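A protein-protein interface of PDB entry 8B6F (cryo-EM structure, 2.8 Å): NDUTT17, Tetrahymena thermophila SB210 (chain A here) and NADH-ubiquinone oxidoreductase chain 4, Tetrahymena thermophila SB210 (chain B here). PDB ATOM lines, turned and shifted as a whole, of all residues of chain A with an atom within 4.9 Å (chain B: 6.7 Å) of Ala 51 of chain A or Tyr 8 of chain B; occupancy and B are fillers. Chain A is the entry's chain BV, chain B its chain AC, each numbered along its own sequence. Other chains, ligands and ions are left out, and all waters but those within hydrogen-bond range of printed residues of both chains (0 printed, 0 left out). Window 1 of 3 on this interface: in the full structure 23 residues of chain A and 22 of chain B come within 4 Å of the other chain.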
ATOM      1  N   HIS A  44      23.466 -12.185  20.532  1.00  0.00           N
ATOM      2  CA  HIS A  44      23.219 -13.585  20.858  1.00  0.00           C
ATOM      3  C   HIS A  44      23.825 -13.943  22.208  1.00  0.00           C
ATOM      4  O   HIS A  44      23.191 -14.624  23.022  1.00  0.00           O
ATOM      5  CB  HIS A  44      23.789 -14.490  19.766  1.00  0.00           C
ATOM      6  CG  HIS A  44      23.039 -14.423  18.474  1.00  0.00           C
ATOM      7  ND1 HIS A  44      21.933 -15.204  18.216  1.00  0.00           N
ATOM      8  CD2 HIS A  44      23.234 -13.670  17.367  1.00  0.00           C
ATOM      9  CE1 HIS A  44      21.480 -14.934  17.005  1.00  0.00           C
ATOM     10  NE2 HIS A  44      22.251 -14.007  16.468  1.00  0.00           N
ATOM     11  N   ALA A  47      21.749 -12.440  25.016  1.00  0.00           N
ATOM     12  CA  ALA A  47      20.513 -13.195  25.191  1.00  0.00           C
ATOM     13  C   ALA A  47      20.771 -14.508  25.917  1.00  0.00           C
ATOM     14  O   ALA A  47      20.006 -14.896  26.806  1.00  0.00           O
ATOM     15  CB  ALA A  47      19.861 -13.450  23.833  1.00  0.00           C
ATOM     16  N   ILE A  48      21.847 -15.209  25.549  1.00  0.00           N
ATOM     17  CA  ILE A  48      22.178 -16.471  26.205  1.00  0.00           C
ATOM     18  C   ILE A  48      22.496 -16.240  27.675  1.00  0.00           C
ATOM     19  O   ILE A  48      22.048 -16.994  28.547  1.00  0.00           O
ATOM     20  CB  ILE A  48      23.347 -17.158  25.477  1.00  0.00           C
ATOM     21  CG1 ILE A  48      22.903 -17.631  24.098  1.00  0.00           C
ATOM     22  CG2 ILE A  48      23.863 -18.346  26.279  1.00  0.00           C
ATOM     23  CD1 ILE A  48      24.043 -18.011  23.193  1.00  0.00           C
ATOM     24  N   LYS A  49      23.261 -15.190  27.978  1.00  0.00           N
ATOM     25  CA  LYS A  49      23.598 -14.907  29.368  1.00  0.00           C
ATOM     26  C   LYS A  49      22.341 -14.640  30.183  1.00  0.00           C
ATOM     27  O   LYS A  49      22.186 -15.157  31.295  1.00  0.00           O
ATOM     28  CB  LYS A  49      24.553 -13.715  29.442  1.00  0.00           C
ATOM     29  CG  LYS A  49      25.117 -13.469  30.834  1.00  0.00           C
ATOM     30  CD  LYS A  49      25.895 -12.164  30.911  1.00  0.00           C
ATOM     31  CE  LYS A  49      24.965 -10.962  30.896  1.00  0.00           C
ATOM     32  NZ  LYS A  49      25.703  -9.688  31.112  1.00  0.00           N
ATOM     33  N   LEU A  50      21.428 -13.833  29.645  1.00  0.00           N
ATOM     34  CA  LEU A  50      20.180 -13.564  30.348  1.00  0.00           C
ATOM     35  C   LEU A  50      19.369 -14.839  30.524  1.00  0.00           C
ATOM     36  O   LEU A  50      18.754 -15.054  31.575  1.00  0.00           O
ATOM     37  CB  LEU A  50      19.369 -12.514  29.591  1.00  0.00           C
ATOM     38  CG  LEU A  50      19.934 -11.092  29.607  1.00  0.00           C
ATOM     39  CD1 LEU A  50      19.150 -10.207  28.658  1.00  0.00           C
ATOM     40  CD2 LEU A  50      19.918 -10.514  31.011  1.00  0.00           C
ATOM     41  N   ALA A  51      19.347 -15.697  29.501  1.00  0.00           N
ATOM     42  CA  ALA A  51      18.598 -16.945  29.600  1.00  0.00           C
ATOM     43  C   ALA A  51      19.156 -17.833  30.703  1.00  0.00           C
ATOM     44  O   ALA A  51      18.404 -18.379  31.517  1.00  0.00           O
ATOM     45  CB  ALA A  51      18.627 -17.676  28.258  1.00  0.00           C
ATOM     46  N   GLN A  52      20.480 -17.986  30.749  1.00  0.00           N
ATOM     47  CA  GLN A  52      21.090 -18.818  31.781  1.00  0.00           C
ATOM     48  C   GLN A  52      20.834 -18.244  33.168  1.00  0.00           C
ATOM     49  O   GLN A  52      20.513 -18.984  34.103  1.00  0.00           O
ATOM     50  CB  GLN A  52      22.588 -18.952  31.522  1.00  0.00           C
ATOM     51  CG  GLN A  52      22.914 -19.665  30.221  1.00  0.00           C
ATOM     52  CD  GLN A  52      24.404 -19.800  29.978  1.00  0.00           C
ATOM     53  OE1 GLN A  52      24.859 -20.797  29.422  1.00  0.00           O
ATOM     54  NE2 GLN A  52      25.172 -18.793  30.381  1.00  0.00           N
ATOM     55  N   GLN A  53      20.976 -16.927  33.321  1.00  0.00           N
ATOM     56  CA  GLN A  53      20.717 -16.304  34.614  1.00  0.00           C
ATOM     57  C   GLN A  53      19.268 -16.503  35.037  1.00  0.00           C
ATOM     58  O   GLN A  53      18.990 -16.813  36.201  1.00  0.00           O
ATOM     59  CB  GLN A  53      21.057 -14.814  34.563  1.00  0.00           C
ATOM     60  CG  GLN A  53      22.543 -14.523  34.468  1.00  0.00           C
ATOM     61  CD  GLN A  53      22.844 -13.039  34.507  1.00  0.00           C
ATOM     62  OE1 GLN A  53      21.949 -12.218  34.694  1.00  0.00           O
ATOM     63  NE2 GLN A  53      24.114 -12.688  34.331  1.00  0.00           N
ATOM     64  N   ASP A  54      18.330 -16.329  34.106  1.00  0.00           N
ATOM     65  CA  ASP A  54      16.921 -16.516  34.436  1.00  0.00           C
ATOM     66  C   ASP A  54      16.638 -17.954  34.846  1.00  0.00           C
ATOM     67  O   ASP A  54      15.903 -18.196  35.810  1.00  0.00           O
ATOM     68  CB  ASP A  54      16.045 -16.113  33.249  1.00  0.00           C
ATOM     69  CG  ASP A  54      16.086 -14.622  32.972  1.00  0.00           C
ATOM     70  OD1 ASP A  54      16.759 -13.892  33.731  1.00  0.00           O
ATOM     71  OD2 ASP A  54      15.444 -14.179  31.997  1.00  0.00           O
ATOM     72  N   PHE A  55      17.209 -18.925  34.131  1.00  0.00           N
ATOM     73  CA  PHE A  55      16.990 -20.318  34.508  1.00  0.00           C
ATOM     74  C   PHE A  55      17.541 -20.604  35.895  1.00  0.00           C
ATOM     75  O   PHE A  55      16.876 -21.251  36.712  1.00  0.00           O
ATOM     76  CB  PHE A  55      17.632 -21.260  33.492  1.00  0.00           C
ATOM     77  CG  PHE A  55      17.599 -22.699  33.916  1.00  0.00           C
ATOM     78  CD1 PHE A  55      16.510 -23.497  33.614  1.00  0.00           C
ATOM     79  CD2 PHE A  55      18.641 -23.248  34.643  1.00  0.00           C
ATOM     80  CE1 PHE A  55      16.467 -24.815  34.012  1.00  0.00           C
ATOM     81  CE2 PHE A  55      18.605 -24.566  35.046  1.00  0.00           C
ATOM     82  CZ  PHE A  55      17.514 -25.351  34.728  1.00  0.00           C
ATOM     83  N   ASN B   3      11.121 -11.737  20.525  1.00  0.00           N
ATOM     84  CA  ASN B   3      12.532 -11.390  20.502  1.00  0.00           C
ATOM     85  C   ASN B   3      13.383 -12.623  20.765  1.00  0.00           C
ATOM     86  O   ASN B   3      12.901 -13.659  21.229  1.00  0.00           O
ATOM     87  CB  ASN B   3      12.862 -10.299  21.529  1.00  0.00           C
ATOM     88  CG  ASN B   3      12.270 -10.585  22.891  1.00  0.00           C
ATOM     89  OD1 ASN B   3      11.807 -11.692  23.158  1.00  0.00           O
ATOM     90  ND2 ASN B   3      12.284  -9.585  23.763  1.00  0.00           N
ATOM     91  N   LEU B   4      14.673 -12.485  20.457  1.00  0.00           N
ATOM     92  CA  LEU B   4      15.616 -13.586  20.603  1.00  0.00           C
ATOM     93  C   LEU B   4      15.758 -14.042  22.049  1.00  0.00           C
ATOM     94  O   LEU B   4      16.165 -15.182  22.289  1.00  0.00           O
ATOM     95  CB  LEU B   4      16.975 -13.162  20.044  1.00  0.00           C
ATOM     96  CG  LEU B   4      18.109 -14.180  20.107  1.00  0.00           C
ATOM     97  CD1 LEU B   4      17.760 -15.434  19.323  1.00  0.00           C
ATOM     98  CD2 LEU B   4      19.386 -13.561  19.582  1.00  0.00           C
ATOM     99  N   ASN B   5      15.429 -13.183  23.014  1.00  0.00           N
ATOM    100  CA  ASN B   5      15.532 -13.574  24.417  1.00  0.00           C
ATOM    101  C   ASN B   5      14.624 -14.757  24.724  1.00  0.00           C
ATOM    102  O   ASN B   5      15.026 -15.689  25.429  1.00  0.00           O
ATOM    103  CB  ASN B   5      15.190 -12.390  25.320  1.00  0.00           C
ATOM    104  CG  ASN B   5      16.250 -11.310  25.291  1.00  0.00           C
ATOM    105  OD1 ASN B   5      17.421 -11.581  25.033  1.00  0.00           O
ATOM    106  ND2 ASN B   5      15.843 -10.075  25.559  1.00  0.00           N
ATOM    107  N   THR B   6      13.394 -14.736  24.209  1.00  0.00           N
ATOM    108  CA  THR B   6      12.480 -15.849  24.442  1.00  0.00           C
ATOM    109  C   THR B   6      13.002 -17.126  23.796  1.00  0.00           C
ATOM    110  O   THR B   6      12.891 -18.213  24.375  1.00  0.00           O
ATOM    111  CB  THR B   6      11.088 -15.511  23.913  1.00  0.00           C
ATOM    112  OG1 THR B   6      10.630 -14.290  24.504  1.00  0.00           O
ATOM    113  CG2 THR B   6      10.103 -16.627  24.248  1.00  0.00           C
ATOM    114  N   ILE B   7      13.556 -17.020  22.587  1.00  0.00           N
ATOM    115  CA  ILE B   7      14.108 -18.196  21.921  1.00  0.00           C
ATOM    116  C   ILE B   7      15.195 -18.830  22.775  1.00  0.00           C
ATOM    117  O   ILE B   7      15.183 -20.038  23.034  1.00  0.00           O
ATOM    118  CB  ILE B   7      14.652 -17.818  20.532  1.00  0.00           C
ATOM    119  CG1 ILE B   7      13.549 -17.205  19.668  1.00  0.00           C
ATOM    120  CG2 ILE B   7      15.316 -19.020  19.878  1.00  0.00           C
ATOM    121  CD1 ILE B   7      14.037 -16.670  18.342  1.00  0.00           C
ATOM    122  N   TYR B   8      16.156 -18.023  23.222  1.00  0.00           N
ATOM    123  CA  TYR B   8      17.270 -18.574  23.982  1.00  0.00           C
ATOM    124  C   TYR B   8      16.827 -19.063  25.350  1.00  0.00           C
ATOM    125  O   TYR B   8      17.362 -20.055  25.853  1.00  0.00           O
ATOM    126  CB  TYR B   8      18.385 -17.542  24.109  1.00  0.00           C
ATOM    127  CG  TYR B   8      19.391 -17.645  22.990  1.00  0.00           C
ATOM    128  CD1 TYR B   8      20.091 -18.824  22.773  1.00  0.00           C
ATOM    129  CD2 TYR B   8      19.639 -16.572  22.151  1.00  0.00           C
ATOM    130  CE1 TYR B   8      21.009 -18.930  21.753  1.00  0.00           C
ATOM    131  CE2 TYR B   8      20.556 -16.668  21.126  1.00  0.00           C
ATOM    132  CZ  TYR B   8      21.238 -17.851  20.932  1.00  0.00           C
ATOM    133  OH  TYR B   8      22.155 -17.955  19.915  1.00  0.00           O
ATOM    134  N   LEU B   9      15.854 -18.394  25.966  1.00  0.00           N
ATOM    135  CA  LEU B   9      15.348 -18.880  27.242  1.00  0.00           C
ATOM    136  C   LEU B   9      14.670 -20.232  27.076  1.00  0.00           C
ATOM    137  O   LEU B   9      14.841 -21.126  27.913  1.00  0.00           O
ATOM    138  CB  LEU B   9      14.388 -17.863  27.855  1.00  0.00           C
ATOM    139  CG  LEU B   9      14.016 -18.154  29.311  1.00  0.00           C
ATOM    140  CD1 LEU B   9      15.220 -18.018  30.229  1.00  0.00           C
ATOM    141  CD2 LEU B   9      12.928 -17.230  29.765  1.00  0.00           C
ATOM    142  N   SER B  10      13.886 -20.400  26.011  1.00  0.00           N
ATOM    143  CA  SER B  10      13.271 -21.696  25.753  1.00  0.00           C
ATOM    144  C   SER B  10      14.329 -22.780  25.596  1.00  0.00           C
ATOM    145  O   SER B  10      14.253 -23.837  26.232  1.00  0.00           O
ATOM    146  CB  SER B  10      12.404 -21.617  24.498  1.00  0.00           C
ATOM    147  OG  SER B  10      11.910 -22.897  24.143  1.00  0.00           O
ATOM    148  N   ARG B  11      15.321 -22.538  24.738  1.00  0.00           N
ATOM    149  CA  ARG B  11      16.346 -23.545  24.489  1.00  0.00           C
ATOM    150  C   ARG B  11      17.138 -23.856  25.752  1.00  0.00           C
ATOM    151  O   ARG B  11      17.431 -25.022  26.040  1.00  0.00           O
ATOM    152  CB  ARG B  11      17.274 -23.077  23.369  1.00  0.00           C
ATOM    153  CG  ARG B  11      16.572 -22.926  22.032  1.00  0.00           C
ATOM    154  CD  ARG B  11      17.557 -22.682  20.908  1.00  0.00           C
ATOM    155  NE  ARG B  11      18.427 -23.831  20.693  1.00  0.00           N
ATOM    156  CZ  ARG B  11      18.098 -24.897  19.975  1.00  0.00           C
ATOM    157  NH1 ARG B  11      16.918 -24.999  19.387  1.00  0.00           N
ATOM    158  NH2 ARG B  11      18.977 -25.887  19.847  1.00  0.00           N
ATOM    159  N   ILE B  12      17.499 -22.823  26.514  1.00  0.00           N
ATOM    160  CA  ILE B  12      18.290 -23.029  27.723  1.00  0.00           C
ATOM    161  C   ILE B  12      17.501 -23.821  28.756  1.00  0.00           C
ATOM    162  O   ILE B  12      18.030 -24.749  29.379  1.00  0.00           O
ATOM    163  CB  ILE B  12      18.764 -21.678  28.288  1.00  0.00           C
ATOM    164  CG1 ILE B  12      19.789 -21.027  27.350  1.00  0.00           C
ATOM    165  CG2 ILE B  12      19.335 -21.846  29.696  1.00  0.00           C
ATOM    166  CD1 ILE B  12      21.128 -21.726  27.280  1.00  0.00           C
ATOM    167  N   PHE B  13      16.228 -23.479  28.955  1.00  0.00           N
ATOM    168  CA  PHE B  13      15.416 -24.218  29.916  1.00  0.00           C
ATOM    169  C   PHE B  13      15.304 -25.683  29.522  1.00  0.00           C
ATOM    170  O   PHE B  13      15.449 -26.577  30.364  1.00  0.00           O
ATOM    171  CB  PHE B  13      14.030 -23.584  30.029  1.00  0.00           C
ATOM    172  CG  PHE B  13      13.863 -22.704  31.231  1.00  0.00           C
ATOM    173  CD1 PHE B  13      14.404 -21.430  31.257  1.00  0.00           C
ATOM    174  CD2 PHE B  13      13.159 -23.150  32.333  1.00  0.00           C
ATOM    175  CE1 PHE B  13      14.248 -20.623  32.363  1.00  0.00           C
ATOM    176  CE2 PHE B  13      12.999 -22.347  33.441  1.00  0.00           C
ATOM    177  CZ  PHE B  13      13.545 -21.081  33.457  1.00  0.00           C
ATOM    178  N   PHE B  16      18.712 -27.392  30.107  1.00  0.00           N
ATOM    179  CA  PHE B  16      19.211 -27.441  31.476  1.00  0.00           C
ATOM    180  C   PHE B  16      18.326 -28.241  32.418  1.00  0.00           C
ATOM    181  O   PHE B  16      18.814 -28.702  33.454  1.00  0.00           O
ATOM    182  CB  PHE B  16      19.378 -26.026  32.035  1.00  0.00           C
ATOM    183  CG  PHE B  16      20.584 -25.292  31.513  1.00  0.00           C
ATOM    184  CD1 PHE B  16      21.351 -25.811  30.481  1.00  0.00           C
ATOM    185  CD2 PHE B  16      20.961 -24.085  32.075  1.00  0.00           C
ATOM    186  CE1 PHE B  16      22.460 -25.135  30.019  1.00  0.00           C
ATOM    187  CE2 PHE B  16      22.069 -23.405  31.616  1.00  0.00           C
ATOM    188  CZ  PHE B  16      22.819 -23.930  30.587  1.00  0.00           C
ATOM    189  N   TYR B  77       7.550 -20.020  21.537  1.00  0.00           N
ATOM    190  CA  TYR B  77       8.598 -20.060  20.523  1.00  0.00           C
ATOM    191  C   TYR B  77       8.082 -20.651  19.216  1.00  0.00           C
ATOM    192  O   TYR B  77       8.335 -20.112  18.133  1.00  0.00           O
ATOM    193  CB  TYR B  77       9.786 -20.870  21.048  1.00  0.00           C
ATOM    194  CG  TYR B  77      10.971 -20.959  20.106  1.00  0.00           C
ATOM    195  CD1 TYR B  77      11.101 -20.098  19.023  1.00  0.00           C
ATOM    196  CD2 TYR B  77      11.956 -21.917  20.302  1.00  0.00           C
ATOM    197  CE1 TYR B  77      12.176 -20.185  18.169  1.00  0.00           C
ATOM    198  CE2 TYR B  77      13.035 -22.013  19.450  1.00  0.00           C
ATOM    199  CZ  TYR B  77      13.136 -21.146  18.384  1.00  0.00           C
ATOM    200  OH  TYR B  77      14.212 -21.235  17.539  1.00  0.00           O
ATOM    201  N   GLU B  98      20.425 -17.870  13.088  1.00  0.00           N
ATOM    202  CA  GLU B  98      21.276 -18.950  13.563  1.00  0.00           C
ATOM    203  C   GLU B  98      21.639 -18.706  15.020  1.00  0.00           C
ATOM    204  O   GLU B  98      22.017 -17.591  15.392  1.00  0.00           O
ATOM    205  CB  GLU B  98      22.536 -19.062  12.705  1.00  0.00           C
ATOM    206  CG  GLU B  98      22.248 -19.428  11.259  1.00  0.00           C
ATOM    207  CD  GLU B  98      23.490 -19.403  10.393  1.00  0.00           C
ATOM    208  OE1 GLU B  98      24.538 -18.924  10.870  1.00  0.00           O
ATOM    209  OE2 GLU B  98      23.418 -19.864   9.234  1.00  0.00           O
ATOM    210  N   LEU B  99      21.522 -19.748  15.837  1.00  0.00           N
ATOM    211  CA  LEU B  99      21.731 -19.661  17.274  1.00  0.00           C
ATOM    212  C   LEU B  99      23.039 -20.340  17.653  1.00  0.00           C
ATOM    213  O   LEU B  99      23.372 -21.405  17.127  1.00  0.00           O
ATOM    214  CB  LEU B  99      20.569 -20.310  18.030  1.00  0.00           C
ATOM    215  CG  LEU B  99      19.174 -19.813  17.651  1.00  0.00           C
ATOM    216  CD1 LEU B  99      18.114 -20.555  18.439  1.00  0.00           C
ATOM    217  CD2 LEU B  99      19.048 -18.317  17.873  1.00  0.00           C
ATOM    218  N   LEU B 100      23.775 -19.721  18.570  1.00  0.00           N
ATOM    219  CA  LEU B 100      25.037 -20.263  19.050  1.00  0.00           C
ATOM    220  C   LEU B 100      24.837 -20.897  20.421  1.00  0.00           C
ATOM    221  O   LEU B 100      24.161 -20.333  21.286  1.00  0.00           O
ATOM    222  CB  LEU B 100      26.109 -19.172  19.117  1.00  0.00           C
ATOM    223  CG  LEU B 100      25.894 -18.029  20.111  1.00  0.00           C
ATOM    224  CD1 LEU B 100      26.653 -18.294  21.399  1.00  0.00           C
ATOM    225  CD2 LEU B 100      26.319 -16.707  19.498  1.00  0.00           C
ATOM    226  N   ASN B 101      25.421 -22.076  20.606  1.00  0.00           N
ATOM    227  CA  ASN B 101      25.206 -22.844  21.821  1.00  0.00           C
ATOM    228  C   ASN B 101      25.928 -22.207  23.007  1.00  0.00           C
ATOM    229  O   ASN B 101      26.909 -21.473  22.858  1.00  0.00           O
ATOM    230  CB  ASN B 101      25.689 -24.280  21.629  1.00  0.00           C
ATOM    231  CG  ASN B 101      25.409 -25.154  22.830  1.00  0.00           C
ATOM    232  OD1 ASN B 101      24.517 -24.862  23.628  1.00  0.00           O
ATOM    233  ND2 ASN B 101      26.172 -26.230  22.969  1.00  0.00           N
ATOM    234  N   ASN B 102      25.424 -22.503  24.203  1.00  0.00           N
ATOM    235  CA  ASN B 102      26.042 -22.018  25.426  1.00  0.00           C
ATOM    236  C   ASN B 102      27.365 -22.735  25.682  1.00  0.00           C
ATOM    237  O   ASN B 102      27.626 -23.825  25.165  1.00  0.00           O
ATOM    238  CB  ASN B 102      25.105 -22.213  26.618  1.00  0.00           C
ATOM    239  CG  ASN B 102      24.673 -23.654  26.793  1.00  0.00           C
ATOM    240  OD1 ASN B 102      25.327 -24.577  26.310  1.00  0.00           O
ATOM    241  ND2 ASN B 102      23.562 -23.855  27.484  1.00  0.00           N
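Printed residues of chain B that touch a printed residue of chain A: Leu 4, Asn 5, Tyr 8, Leu 9, Ile 12, Phe 13, Phe 16, Glu 98, Leu 100 and Asn 102.
Hydrophobic or aromatic side chains of chain B within 4 Å of the printed part of chain A: Leu 4, Tyr 8, Leu 9, Ile 12, Phe 13, Phe 16 and Leu 100.
Printed residues of chain A that touch a printed residue of chain B: His 44, Ala 47, Ile 48, Ala 51, Gln 52, Asp 54 and Phe 55.
Hydrophobic or aromatic side chains of chain A that line the printed part of chain B: His 44, Ala 47, Ile 48, Ala 51 and Phe 55.
Among the printed residues, no Asp or Glu carboxylate lies within 4 Å of a Lys or Arg side-chain nitrogen of the other chain.
The side-chain hydroxyl (OH) of Tyr 8 of chain B sits at hydrogen-bond distance from a ring nitrogen (ND1) of His 44 of chain A (3.2 Å).
OH of Tyr 8 of chain B lies within hydrogen-bond range of N of Leu 100 of chain B (2.7 Å).
The side-chain amide oxygen (OD1) of Asn 102 of chain B lies close to the side-chain amide oxygen (OD1) of Asn 101 of chain B (2.8 Å).
Of chain B, only Tyr 8 (3.6 Å), Leu 9 (3.5 Å) and Ile 12 (3.7 Å) come within 4 Å of Ala 51 of chain A.
Of chain A, only His 44, Ala 47, Ile 48 and Ala 51 come within 4 Å of Tyr 8 of chain B.
Of the printed residues of chain B, Asp 54 of chain A touches Leu 9 (3.7 Å).
Of the printed residues of chain B, Ala 47 of chain A touches Asn 5 (3.3 Å) and Tyr 8 (3.6 Å).
Printed residues of chain A within 4 Å of Leu 100 of chain B: His 44 (3.4 Å) and Ile 48 (3.0 Å).
Printed residues of chain A within 4 Å of Phe 16 of chain B: Gln 52 (3.9 Å) and Phe 55 (3.3 Å).
Printed residues of chain A within 4 Å of Glu 98 of chain B: His 44 (3.2 Å).
The nearest residue of chain B that does not touch Ala 51 of chain A is Phe 13 of chain B (4.8 Å).
The nearest printed residue of chain A that does not touch Tyr 8 of chain B is Gln 52 of chain A (6.2 Å).
Among the printed residues, pairs that only touch across the chains: His 44 of chain A with Leu 4 of chain B, His 44 of chain A with Glu 98 of chain B, His 44 of chain A with Leu 100 of chain B, Ala 47 of chain A with Asn 5 of chain B, Ala 47 of chain A with Tyr 8 of chain B, Ile 48 of chain A with Tyr 8 of chain B, Ile 48 of chain A with Leu 100 of chain B, Ala 51 of chain A with Tyr 8 of chain B, Ala 51 of chain A with Leu 9 of chain B, Ala 51 of chain A with Ile 12 of chain B, Gln 52 of chain A with Phe 16 of chain B, Gln 52 of chain A with Asn 102 of chain B, Asp 54 of chain A with Leu 9 of chain B, Phe 55 of chain A with Phe 13 of chain B and Phe 55 of chain A with Phe 16 of chain B.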
